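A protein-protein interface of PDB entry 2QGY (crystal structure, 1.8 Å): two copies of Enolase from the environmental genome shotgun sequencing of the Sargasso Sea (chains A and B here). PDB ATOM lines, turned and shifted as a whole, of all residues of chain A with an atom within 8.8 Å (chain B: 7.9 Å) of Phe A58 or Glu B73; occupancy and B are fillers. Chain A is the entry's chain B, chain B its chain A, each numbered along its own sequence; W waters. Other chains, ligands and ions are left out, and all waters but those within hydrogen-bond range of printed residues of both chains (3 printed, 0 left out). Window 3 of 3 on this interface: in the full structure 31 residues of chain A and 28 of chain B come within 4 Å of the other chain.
The side-chain carboxylate (OD2) of Asp A100 is in salt-bridge range of the guanidinium group (NH2) of Arg A59 (2.7 Å). The guanidinium group of Arg B72 lies within salt-bridge range of the side-chain carboxylate of Glu B69 (3.0 Å). O of Glu B73 lies close to OD1 of Asn B76 (2.9 Å). OE1 of Glu A60 is in hydrogen-bond range of N of Phe A58, at 3.2 Å. The side-chain amino group (NZ) of Lys B88 lies within salt-bridge range of the side-chain carboxylate (OE2) of Glu B73 (3.0 Å).
Among the printed residues, merely in contact across the chains: Phe A58 with Glu B73 (3.4 Å), Arg A59 with Phe B101 (3.5 Å), Phe A58 with Glu B69 (3.5 Å), Lys A61 with Ile B65 (3.6 Å), Gly A62 with Ile B65 (3.6 Å), Phe A58 with Leu B92 (3.6 Å), Asp A100 with Phe B101 (3.8 Å) and Gly A62 with Gly B62 (3.8 Å).
No residue of chain B comes within 4 Å of Asn A57. Phe A58 touches three residues of chain B. Printed residues of chain B within 4 Å of Arg A59: Phe B101. Of the printed residues of chain A, Gly B62 touches Gly A62 (3.8 Å). Of the printed residues of chain A, Ile B65 touches Lys A61 and Gly A62. Printed residues of chain A within 4 Å of Glu B69: Phe A58 (3.5 Å). Glu B73 touches just one residue of chain A: Phe A58. The nearest residue of chain A that does not touch Glu B73 is Asn A57 (6.9 Å). The nearest printed residue of chain A that does not touch Glu B69 is Lys A61 (4.9 Å).
Of the 23 printed residues of chain B, 6 touch a printed residue of chain A. Printed residues of chain B that touch a printed residue of chain A: Gly B62, Ile B65, Glu B69, Glu B73, Leu B92 and Phe B101. Along chain B the printed residues that touch a printed residue of chain A span positions 62 to 101. Along chain A the printed residues that touch a printed residue of chain B span positions 58 to 100.
Gly B62 touches its own counterpart, Gly A62. 2 positions are printed for both chains.
Water W3 lies within hydrogen-bond range of the side-chain carboxylate of Asp A100 (2.5 Å) and the backbone NH of Phe B101 (3.0 Å). Water W2 bridges the backbone carbonyl oxygen of Leu B92 (2.7 Å) and the side-chain amide oxygen of Asn A57 (2.8 Å). Water W1 lies within hydrogen-bond range of the backbone carbonyl oxygen (O) of Asn A57 (2.8 Å), the guanidinium group (NH1) of Arg A59 (2.9 Å) and the backbone carbonyl oxygen (O) of Leu B92 (3.2 Å).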
ATOM      1  N   LYS A  35      -0.783  32.712  -1.494  1.00  0.00           N
ATOM      2  CA  LYS A  35      -1.487  33.496  -0.502  1.00  0.00           C
ATOM      3  C   LYS A  35      -0.813  33.113   0.828  1.00  0.00           C
ATOM      4  O   LYS A  35      -0.599  31.927   1.086  1.00  0.00           O
ATOM      5  CB  LYS A  35      -2.976  33.126  -0.478  1.00  0.00           C
ATOM      6  CG  LYS A  35      -3.735  33.410  -1.783  1.00  0.00           C
ATOM      7  CD  LYS A  35      -5.247  33.229  -1.602  1.00  0.00           C
ATOM      8  CE  LYS A  35      -6.054  33.676  -2.842  1.00  0.00           C
ATOM      9  NZ  LYS A  35      -5.647  32.863  -4.041  1.00  0.00           N
ATOM     10  N   ILE A  37      -0.714  33.331   5.095  1.00  0.00           N
ATOM     11  CA  ILE A  37      -1.654  33.505   6.200  1.00  0.00           C
ATOM     12  C   ILE A  37      -0.807  33.988   7.376  1.00  0.00           C
ATOM     13  O   ILE A  37       0.020  33.235   7.929  1.00  0.00           O
ATOM     14  CB  ILE A  37      -2.379  32.188   6.591  1.00  0.00           C
ATOM     15  CG1 ILE A  37      -3.240  31.642   5.432  1.00  0.00           C
ATOM     16  CG2 ILE A  37      -3.235  32.422   7.810  1.00  0.00           C
ATOM     17  CD1 ILE A  37      -3.527  30.138   5.573  1.00  0.00           C
ATOM     18  N   SER A  55       0.349  27.885   4.247  1.00  0.00           N
ATOM     19  CA  SER A  55      -0.863  28.074   3.490  1.00  0.00           C
ATOM     20  C   SER A  55      -0.987  27.025   2.392  1.00  0.00           C
ATOM     21  O   SER A  55      -0.033  26.702   1.736  1.00  0.00           O
ATOM     22  CB  SER A  55      -0.850  29.474   2.896  1.00  0.00           C
ATOM     23  OG  SER A  55      -1.999  29.645   2.102  1.00  0.00           O
ATOM     24  N   ILE A  56      -2.184  26.498   2.212  1.00  0.00           N
ATOM     25  CA  ILE A  56      -2.434  25.404   1.261  1.00  0.00           C
ATOM     26  C   ILE A  56      -3.603  25.839   0.366  1.00  0.00           C
ATOM     27  O   ILE A  56      -4.621  26.296   0.862  1.00  0.00           O
ATOM     28  CB  ILE A  56      -2.801  24.100   2.005  1.00  0.00           C
ATOM     29  CG1 ILE A  56      -1.874  23.857   3.215  1.00  0.00           C
ATOM     30  CG2 ILE A  56      -2.728  22.891   1.062  1.00  0.00           C
ATOM     31  CD1 ILE A  56      -2.402  22.736   4.127  1.00  0.00           C
ATOM     32  N   ASN A  57      -3.443  25.668  -0.948  1.00  0.00           N
ATOM     33  CA  ASN A  57      -4.411  26.122  -1.961  1.00  0.00           C
ATOM     34  C   ASN A  57      -5.809  25.591  -1.660  1.00  0.00           C
ATOM     35  O   ASN A  57      -6.006  24.379  -1.453  1.00  0.00           O
ATOM     36  CB  ASN A  57      -3.931  25.649  -3.349  1.00  0.00           C
ATOM     37  CG  ASN A  57      -4.600  26.377  -4.510  1.00  0.00           C
ATOM     38  OD1 ASN A  57      -4.587  25.866  -5.647  1.00  0.00           O
ATOM     39  ND2 ASN A  57      -5.159  27.554  -4.264  1.00  0.00           N
ATOM     40  N   PHE A  58      -6.769  26.516  -1.580  1.00  0.00           N
ATOM     41  CA  PHE A  58      -8.206  26.239  -1.313  1.00  0.00           C
ATOM     42  C   PHE A  58      -8.535  25.995   0.155  1.00  0.00           C
ATOM     43  O   PHE A  58      -9.693  25.776   0.518  1.00  0.00           O
ATOM     44  CB  PHE A  58      -8.800  25.132  -2.212  1.00  0.00           C
ATOM     45  CG  PHE A  58      -8.694  25.438  -3.684  1.00  0.00           C
ATOM     46  CD1 PHE A  58      -9.571  26.351  -4.282  1.00  0.00           C
ATOM     47  CD2 PHE A  58      -7.700  24.842  -4.469  1.00  0.00           C
ATOM     48  CE1 PHE A  58      -9.458  26.648  -5.659  1.00  0.00           C
ATOM     49  CE2 PHE A  58      -7.585  25.131  -5.818  1.00  0.00           C
ATOM     50  CZ  PHE A  58      -8.452  26.032  -6.417  1.00  0.00           C
ATOM     51  N   ARG A  59      -7.519  26.040   0.998  1.00  0.00           N
ATOM     52  CA  ARG A  59      -7.729  25.762   2.404  1.00  0.00           C
ATOM     53  C   ARG A  59      -7.317  26.933   3.302  1.00  0.00           C
ATOM     54  O   ARG A  59      -7.406  26.838   4.536  1.00  0.00           O
ATOM     55  CB  ARG A  59      -6.937  24.494   2.739  1.00  0.00           C
ATOM     56  CG  ARG A  59      -7.482  23.297   1.972  1.00  0.00           C
ATOM     57  CD  ARG A  59      -6.342  22.459   1.380  1.00  0.00           C
ATOM     58  NE  ARG A  59      -5.771  21.555   2.366  1.00  0.00           N
ATOM     59  CZ  ARG A  59      -5.095  20.442   2.057  1.00  0.00           C
ATOM     60  NH1 ARG A  59      -4.859  20.102   0.792  1.00  0.00           N
ATOM     61  NH2 ARG A  59      -4.650  19.668   3.033  1.00  0.00           N
ATOM     62  N   GLU A  60      -6.868  28.032   2.694  1.00  0.00           N
ATOM     63  CA  GLU A  60      -6.402  29.182   3.465  1.00  0.00           C
ATOM     64  C   GLU A  60      -7.467  29.737   4.412  1.00  0.00           C
ATOM     65  O   GLU A  60      -7.177  29.993   5.583  1.00  0.00           O
ATOM     66  CB  GLU A  60      -5.906  30.285   2.555  1.00  0.00           C
ATOM     67  CG  GLU A  60      -4.858  29.838   1.533  1.00  0.00           C
ATOM     68  CD  GLU A  60      -5.457  29.487   0.175  1.00  0.00           C
ATOM     69  OE1 GLU A  60      -6.665  29.211   0.107  1.00  0.00           O
ATOM     70  OE2 GLU A  60      -4.692  29.466  -0.814  1.00  0.00           O
ATOM     71  N   LYS A  61      -8.689  29.928   3.906  1.00  0.00           N
ATOM     72  CA  LYS A  61      -9.784  30.423   4.765  1.00  0.00           C
ATOM     73  C   LYS A  61     -10.159  29.406   5.848  1.00  0.00           C
ATOM     74  O   LYS A  61     -10.467  29.759   6.982  1.00  0.00           O
ATOM     75  CB  LYS A  61     -11.030  30.800   3.947  1.00  0.00           C
ATOM     76  CG  LYS A  61     -11.957  31.713   4.783  1.00  0.00           C
ATOM     77  CD  LYS A  61     -13.035  32.437   3.987  1.00  0.00           C
ATOM     78  CE  LYS A  61     -14.071  33.032   4.960  1.00  0.00           C
ATOM     79  NZ  LYS A  61     -14.963  32.006   5.574  1.00  0.00           N
ATOM     80  N   GLY A  62     -10.115  28.136   5.480  1.00  0.00           N
ATOM     81  CA  GLY A  62     -10.407  27.064   6.416  1.00  0.00           C
ATOM     82  C   GLY A  62      -9.353  27.035   7.518  1.00  0.00           C
ATOM     83  O   GLY A  62      -9.684  26.872   8.696  1.00  0.00           O
ATOM     84  N   ILE A  63      -8.095  27.238   7.161  1.00  0.00           N
ATOM     85  CA  ILE A  63      -7.032  27.292   8.181  1.00  0.00           C
ATOM     86  C   ILE A  63      -7.260  28.495   9.117  1.00  0.00           C
ATOM     87  O   ILE A  63      -7.119  28.410  10.367  1.00  0.00           O
ATOM     88  CB  ILE A  63      -5.638  27.329   7.497  1.00  0.00           C
ATOM     89  CG1 ILE A  63      -5.352  25.944   6.844  1.00  0.00           C
ATOM     90  CG2 ILE A  63      -4.491  27.768   8.472  1.00  0.00           C
ATOM     91  CD1 ILE A  63      -4.324  25.971   5.748  1.00  0.00           C
ATOM     92  N   ASP A 100      -3.615  20.909   7.586  1.00  0.00           N
ATOM     93  CA  ASP A 100      -4.380  22.127   7.823  1.00  0.00           C
ATOM     94  C   ASP A 100      -4.421  22.499   9.313  1.00  0.00           C
ATOM     95  O   ASP A 100      -4.202  23.662   9.687  1.00  0.00           O
ATOM     96  CB  ASP A 100      -5.776  22.022   7.218  1.00  0.00           C
ATOM     97  CG  ASP A 100      -5.733  21.608   5.762  1.00  0.00           C
ATOM     98  OD1 ASP A 100      -5.851  22.515   4.916  1.00  0.00           O
ATOM     99  OD2 ASP A 100      -5.566  20.391   5.462  1.00  0.00           O
ATOM    100  N   LEU B  13     -22.455  22.104 -11.250  1.00  0.00           N
ATOM    101  CA  LEU B  13     -23.150  22.136  -9.971  1.00  0.00           C
ATOM    102  C   LEU B  13     -23.727  23.501  -9.782  1.00  0.00           C
ATOM    103  O   LEU B  13     -23.107  24.491 -10.168  1.00  0.00           O
ATOM    104  CB  LEU B  13     -22.195  21.813  -8.808  1.00  0.00           C
ATOM    105  CG  LEU B  13     -21.387  20.521  -8.897  1.00  0.00           C
ATOM    106  CD1 LEU B  13     -20.539  20.343  -7.647  1.00  0.00           C
ATOM    107  CD2 LEU B  13     -22.307  19.278  -9.083  1.00  0.00           C
ATOM    108  N   GLY B  62     -14.068  24.946   9.874  1.00  0.00           N
ATOM    109  CA  GLY B  62     -12.924  24.887   8.961  1.00  0.00           C
ATOM    110  C   GLY B  62     -13.166  23.883   7.846  1.00  0.00           C
ATOM    111  O   GLY B  62     -12.939  24.179   6.673  1.00  0.00           O
ATOM    112  N   ILE B  63     -13.677  22.711   8.208  1.00  0.00           N
ATOM    113  CA  ILE B  63     -13.994  21.685   7.222  1.00  0.00           C
ATOM    114  C   ILE B  63     -15.072  22.209   6.249  1.00  0.00           C
ATOM    115  O   ILE B  63     -14.945  22.079   5.008  1.00  0.00           O
ATOM    116  CB  ILE B  63     -14.396  20.371   7.921  1.00  0.00           C
ATOM    117  CG1 ILE B  63     -13.170  19.744   8.648  1.00  0.00           C
ATOM    118  CG2 ILE B  63     -15.019  19.368   6.928  1.00  0.00           C
ATOM    119  CD1 ILE B  63     -13.576  18.678   9.638  1.00  0.00           C
ATOM    120  N   ILE B  65     -15.852  25.294   5.429  1.00  0.00           N
ATOM    121  CA  ILE B  65     -15.280  26.312   4.569  1.00  0.00           C
ATOM    122  C   ILE B  65     -14.450  25.727   3.425  1.00  0.00           C
ATOM    123  O   ILE B  65     -14.536  26.189   2.279  1.00  0.00           O
ATOM    124  CB  ILE B  65     -14.494  27.360   5.405  1.00  0.00           C
ATOM    125  CG1 ILE B  65     -15.457  28.166   6.292  1.00  0.00           C
ATOM    126  CG2 ILE B  65     -13.599  28.247   4.512  1.00  0.00           C
ATOM    127  CD1 ILE B  65     -16.617  28.834   5.562  1.00  0.00           C
ATOM    128  N   ILE B  66     -13.696  24.674   3.724  1.00  0.00           N
ATOM    129  CA  ILE B  66     -12.977  23.924   2.702  1.00  0.00           C
ATOM    130  C   ILE B  66     -13.925  23.264   1.700  1.00  0.00           C
ATOM    131  O   ILE B  66     -13.721  23.391   0.491  1.00  0.00           O
ATOM    132  CB  ILE B  66     -12.009  22.884   3.335  1.00  0.00           C
ATOM    133  CG1 ILE B  66     -10.884  23.614   4.074  1.00  0.00           C
ATOM    134  CG2 ILE B  66     -11.421  21.966   2.248  1.00  0.00           C
ATOM    135  CD1 ILE B  66     -10.083  22.631   4.974  1.00  0.00           C
ATOM    136  N   ILE B  67     -14.968  22.586   2.183  1.00  0.00           N
ATOM    137  CA  ILE B  67     -15.978  22.071   1.272  1.00  0.00           C
ATOM    138  C   ILE B  67     -16.518  23.190   0.380  1.00  0.00           C
ATOM    139  O   ILE B  67     -16.665  23.001  -0.831  1.00  0.00           O
ATOM    140  CB  ILE B  67     -17.190  21.434   2.047  1.00  0.00           C
ATOM    141  CG1 ILE B  67     -16.723  20.175   2.786  1.00  0.00           C
ATOM    142  CG2 ILE B  67     -18.358  21.093   1.082  1.00  0.00           C
ATOM    143  CD1 ILE B  67     -17.739  19.639   3.815  1.00  0.00           C
ATOM    144  N   LYS B  68     -16.834  24.334   0.978  1.00  0.00           N
ATOM    145  CA  LYS B  68     -17.353  25.462   0.216  1.00  0.00           C
ATOM    146  C   LYS B  68     -16.356  25.926  -0.858  1.00  0.00           C
ATOM    147  O   LYS B  68     -16.749  26.188  -2.011  1.00  0.00           O
ATOM    148  CB  LYS B  68     -17.705  26.646   1.141  1.00  0.00           C
ATOM    149  CG  LYS B  68     -18.248  27.863   0.349  1.00  0.00           C
ATOM    150  CD  LYS B  68     -18.884  28.931   1.241  1.00  0.00           C
ATOM    151  CE  LYS B  68     -17.969  30.150   1.419  1.00  0.00           C
ATOM    152  NZ  LYS B  68     -18.627  31.333   2.127  1.00  0.00           N
ATOM    153  N   GLU B  69     -15.074  26.002  -0.503  1.00  0.00           N
ATOM    154  CA  GLU B  69     -14.083  26.453  -1.491  1.00  0.00           C
ATOM    155  C   GLU B  69     -13.859  25.464  -2.618  1.00  0.00           C
ATOM    156  O   GLU B  69     -13.676  25.848  -3.807  1.00  0.00           O
ATOM    157  CB  GLU B  69     -12.753  26.809  -0.834  1.00  0.00           C
ATOM    158  CG  GLU B  69     -12.775  28.087   0.009  1.00  0.00           C
ATOM    159  CD  GLU B  69     -13.238  29.333  -0.759  1.00  0.00           C
ATOM    160  OE1 GLU B  69     -12.827  29.512  -1.926  1.00  0.00           O
ATOM    161  OE2 GLU B  69     -14.005  30.142  -0.189  1.00  0.00           O
ATOM    162  N   LEU B  70     -13.879  24.182  -2.259  1.00  0.00           N
ATOM    163  CA  LEU B  70     -13.774  23.126  -3.254  1.00  0.00           C
ATOM    164  C   LEU B  70     -14.990  23.159  -4.174  1.00  0.00           C
ATOM    165  O   LEU B  70     -14.869  23.034  -5.387  1.00  0.00           O
ATOM    166  CB  LEU B  70     -13.612  21.769  -2.590  1.00  0.00           C
ATOM    167  CG  LEU B  70     -12.263  21.584  -1.883  1.00  0.00           C
ATOM    168  CD1 LEU B  70     -12.215  20.247  -1.127  1.00  0.00           C
ATOM    169  CD2 LEU B  70     -11.082  21.684  -2.826  1.00  0.00           C
ATOM    170  N   PHE B  71     -16.160  23.374  -3.591  1.00  0.00           N
ATOM    171  CA  PHE B  71     -17.365  23.421  -4.369  1.00  0.00           C
ATOM    172  C   PHE B  71     -17.293  24.513  -5.430  1.00  0.00           C
ATOM    173  O   PHE B  71     -17.617  24.260  -6.585  1.00  0.00           O
ATOM    174  CB  PHE B  71     -18.574  23.627  -3.468  1.00  0.00           C
ATOM    175  CG  PHE B  71     -19.830  23.949  -4.212  1.00  0.00           C
ATOM    176  CD1 PHE B  71     -20.584  22.929  -4.783  1.00  0.00           C
ATOM    177  CD2 PHE B  71     -20.262  25.262  -4.333  1.00  0.00           C
ATOM    178  CE1 PHE B  71     -21.740  23.211  -5.465  1.00  0.00           C
ATOM    179  CE2 PHE B  71     -21.428  25.546  -5.028  1.00  0.00           C
ATOM    180  CZ  PHE B  71     -22.152  24.522  -5.589  1.00  0.00           C
ATOM    181  N   ARG B  72     -16.871  25.707  -5.034  1.00  0.00           N
ATOM    182  CA  ARG B  72     -16.766  26.846  -5.948  1.00  0.00           C
ATOM    183  C   ARG B  72     -15.839  26.500  -7.100  1.00  0.00           C
ATOM    184  O   ARG B  72     -16.144  26.783  -8.273  1.00  0.00           O
ATOM    185  CB  ARG B  72     -16.248  28.080  -5.221  1.00  0.00           C
ATOM    186  CG  ARG B  72     -17.259  28.760  -4.318  1.00  0.00           C
ATOM    187  CD  ARG B  72     -16.685  30.076  -3.787  1.00  0.00           C
ATOM    188  NE  ARG B  72     -17.530  30.650  -2.741  1.00  0.00           N
ATOM    189  CZ  ARG B  72     -17.108  31.498  -1.800  1.00  0.00           C
ATOM    190  NH1 ARG B  72     -15.832  31.867  -1.739  1.00  0.00           N
ATOM    191  NH2 ARG B  72     -17.966  31.968  -0.901  1.00  0.00           N
ATOM    192  N   GLU B  73     -14.716  25.873  -6.779  1.00  0.00           N
ATOM    193  CA  GLU B  73     -13.740  25.514  -7.804  1.00  0.00           C
ATOM    194  C   GLU B  73     -14.281  24.490  -8.799  1.00  0.00           C
ATOM    195  O   GLU B  73     -14.028  24.577  -9.992  1.00  0.00           O
ATOM    196  CB  GLU B  73     -12.441  25.026  -7.145  1.00  0.00           C
ATOM    197  CG  GLU B  73     -11.337  24.641  -8.125  1.00  0.00           C
ATOM    198  CD  GLU B  73     -10.785  25.823  -8.947  1.00  0.00           C
ATOM    199  OE1 GLU B  73     -11.068  27.004  -8.629  1.00  0.00           O
ATOM    200  OE2 GLU B  73     -10.040  25.554  -9.914  1.00  0.00           O
ATOM    201  N   ILE B  74     -15.042  23.525  -8.316  1.00  0.00           N
ATOM    202  CA  ILE B  74     -15.524  22.464  -9.187  1.00  0.00           C
ATOM    203  C   ILE B  74     -16.879  22.738  -9.850  1.00  0.00           C
ATOM    204  O   ILE B  74     -17.258  22.008 -10.762  1.00  0.00           O
ATOM    205  CB  ILE B  74     -15.589  21.120  -8.444  1.00  0.00           C
ATOM    206  CG1 ILE B  74     -16.693  21.171  -7.379  1.00  0.00           C
ATOM    207  CG2 ILE B  74     -14.209  20.794  -7.848  1.00  0.00           C
ATOM    208  CD1 ILE B  74     -17.234  19.823  -6.956  1.00  0.00           C
ATOM    209  N   SER B  75     -17.591  23.774  -9.399  1.00  0.00           N
ATOM    210  CA  SER B  75     -18.997  23.989  -9.812  1.00  0.00           C
ATOM    211  C   SER B  75     -19.187  24.407 -11.278  1.00  0.00           C
ATOM    212  O   SER B  75     -20.297  24.290 -11.821  1.00  0.00           O
ATOM    213  CB  SER B  75     -19.697  24.998  -8.893  1.00  0.00           C
ATOM    214  OG  SER B  75     -19.086  26.272  -8.979  1.00  0.00           O
ATOM    215  N   ASN B  76     -18.115  24.894 -11.899  1.00  0.00           N
ATOM    216  CA  ASN B  76     -18.164  25.390 -13.282  1.00  0.00           C
ATOM    217  C   ASN B  76     -17.616  24.384 -14.298  1.00  0.00           C
ATOM    218  O   ASN B  76     -17.566  24.671 -15.499  1.00  0.00           O
ATOM    219  CB  ASN B  76     -17.413  26.733 -13.395  1.00  0.00           C
ATOM    220  CG  ASN B  76     -16.150  26.791 -12.511  1.00  0.00           C
ATOM    221  OD1 ASN B  76     -15.896  25.894 -11.700  1.00  0.00           O
ATOM    222  ND2 ASN B  76     -15.364  27.857 -12.667  1.00  0.00           N
ATOM    223  N   ILE B  77     -17.198  23.215 -13.804  1.00  0.00           N
ATOM    224  CA  ILE B  77     -16.679  22.151 -14.655  1.00  0.00           C
ATOM    225  C   ILE B  77     -17.865  21.521 -15.383  1.00  0.00           C
ATOM    226  O   ILE B  77     -18.680  20.833 -14.771  1.00  0.00           O
ATOM    227  CB  ILE B  77     -15.894  21.076 -13.837  1.00  0.00           C
ATOM    228  CG1 ILE B  77     -14.687  21.707 -13.110  1.00  0.00           C
ATOM    229  CG2 ILE B  77     -15.482  19.919 -14.738  1.00  0.00           C
ATOM    230  CD1 ILE B  77     -13.767  20.711 -12.382  1.00  0.00           C
ATOM    231  N   LEU B  80     -18.377  17.415 -15.349  1.00  0.00           N
ATOM    232  CA  LEU B  80     -17.994  16.825 -14.055  1.00  0.00           C
ATOM    233  C   LEU B  80     -18.495  15.387 -13.864  1.00  0.00           C
ATOM    234  O   LEU B  80     -19.629  15.050 -14.217  1.00  0.00           O
ATOM    235  CB  LEU B  80     -18.487  17.712 -12.908  1.00  0.00           C
ATOM    236  CG  LEU B  80     -18.016  17.400 -11.481  1.00  0.00           C
ATOM    237  CD1 LEU B  80     -16.502  17.600 -11.333  1.00  0.00           C
ATOM    238  CD2 LEU B  80     -18.781  18.276 -10.484  1.00  0.00           C
ATOM    239  N   LYS B  88      -9.268  16.007 -10.142  1.00  0.00           N
ATOM    240  CA  LYS B  88      -9.077  17.414  -9.842  1.00  0.00           C
ATOM    241  C   LYS B  88      -8.569  17.595  -8.408  1.00  0.00           C
ATOM    242  O   LYS B  88      -7.677  18.398  -8.161  1.00  0.00           O
ATOM    243  CB  LYS B  88     -10.391  18.162 -10.014  1.00  0.00           C
ATOM    244  CG  LYS B  88     -10.380  19.619  -9.552  1.00  0.00           C
ATOM    245  CD  LYS B  88      -9.642  20.516 -10.534  1.00  0.00           C
ATOM    246  CE  LYS B  88      -9.835  21.978 -10.159  1.00  0.00           C
ATOM    247  NZ  LYS B  88      -9.497  22.891 -11.295  1.00  0.00           N
ATOM    248  N   ILE B  89      -9.184  16.878  -7.471  1.00  0.00           N
ATOM    249  CA  ILE B  89      -8.702  16.870  -6.081  1.00  0.00           C
ATOM    250  C   ILE B  89      -7.218  16.480  -6.010  1.00  0.00           C
ATOM    251  O   ILE B  89      -6.432  17.154  -5.339  1.00  0.00           O
ATOM    252  CB  ILE B  89      -9.566  15.938  -5.148  1.00  0.00           C
ATOM    253  CG1 ILE B  89     -10.950  16.540  -4.922  1.00  0.00           C
ATOM    254  CG2 ILE B  89      -8.866  15.703  -3.756  1.00  0.00           C
ATOM    255  CD1 ILE B  89     -10.941  18.010  -4.406  1.00  0.00           C
ATOM    256  N   LEU B  91      -4.957  16.750  -8.271  1.00  0.00           N
ATOM    257  CA  LEU B  91      -4.152  17.843  -8.847  1.00  0.00           C
ATOM    258  C   LEU B  91      -3.980  19.029  -7.883  1.00  0.00           C
ATOM    259  O   LEU B  91      -2.863  19.455  -7.604  1.00  0.00           O
ATOM    260  CB  LEU B  91      -4.743  18.318 -10.184  1.00  0.00           C
ATOM    261  CG  LEU B  91      -4.204  19.650 -10.742  1.00  0.00           C
ATOM    262  CD1 LEU B  91      -2.776  19.519 -11.288  1.00  0.00           C
ATOM    263  CD2 LEU B  91      -5.151  20.252 -11.820  1.00  0.00           C
ATOM    264  N   LEU B  92      -5.089  19.533  -7.346  1.00  0.00           N
ATOM    265  CA  LEU B  92      -5.029  20.707  -6.500  1.00  0.00           C
ATOM    266  C   LEU B  92      -4.414  20.463  -5.117  1.00  0.00           C
ATOM    267  O   LEU B  92      -3.743  21.357  -4.566  1.00  0.00           O
ATOM    268  CB  LEU B  92      -6.391  21.401  -6.439  1.00  0.00           C
ATOM    269  CG  LEU B  92      -7.570  20.814  -5.700  1.00  0.00           C
ATOM    270  CD1 LEU B  92      -7.476  21.231  -4.230  1.00  0.00           C
ATOM    271  CD2 LEU B  92      -8.828  21.423  -6.316  1.00  0.00           C
ATOM    272  N   SER B  93      -4.583  19.258  -4.576  1.00  0.00           N
ATOM    273  CA  SER B  93      -4.026  18.969  -3.239  1.00  0.00           C
ATOM    274  C   SER B  93      -2.517  18.768  -3.248  1.00  0.00           C
ATOM    275  O   SER B  93      -1.858  19.009  -2.240  1.00  0.00           O
ATOM    276  CB  SER B  93      -4.715  17.775  -2.584  1.00  0.00           C
ATOM    277  OG  SER B  93      -4.525  16.590  -3.317  1.00  0.00           O
ATOM    278  N   PHE B 101      -8.949  17.834   5.475  1.00  0.00           N
ATOM    279  CA  PHE B 101      -9.140  17.948   4.037  1.00  0.00           C
ATOM    280  C   PHE B 101      -9.856  16.699   3.495  1.00  0.00           C
ATOM    281  O   PHE B 101     -10.770  16.805   2.666  1.00  0.00           O
ATOM    282  CB  PHE B 101      -7.792  18.162   3.337  1.00  0.00           C
ATOM    283  CG  PHE B 101      -7.890  18.264   1.853  1.00  0.00           C
ATOM    284  CD1 PHE B 101      -8.378  19.444   1.243  1.00  0.00           C
ATOM    285  CD2 PHE B 101      -7.474  17.220   1.049  1.00  0.00           C
ATOM    286  CE1 PHE B 101      -8.463  19.538  -0.142  1.00  0.00           C
ATOM    287  CE2 PHE B 101      -7.550  17.332  -0.334  1.00  0.00           C
ATOM    288  CZ  PHE B 101      -8.043  18.494  -0.920  1.00  0.00           C
HETATM  289  O   HOH W   1      -4.891  21.855  -1.575  1.00  0.00           O
HETATM  290  O   HOH W   2      -2.846  23.660  -5.634  1.00  0.00           O
HETATM  291  O   HOH W   3      -6.212  18.263   6.493  1.00  0.00           O
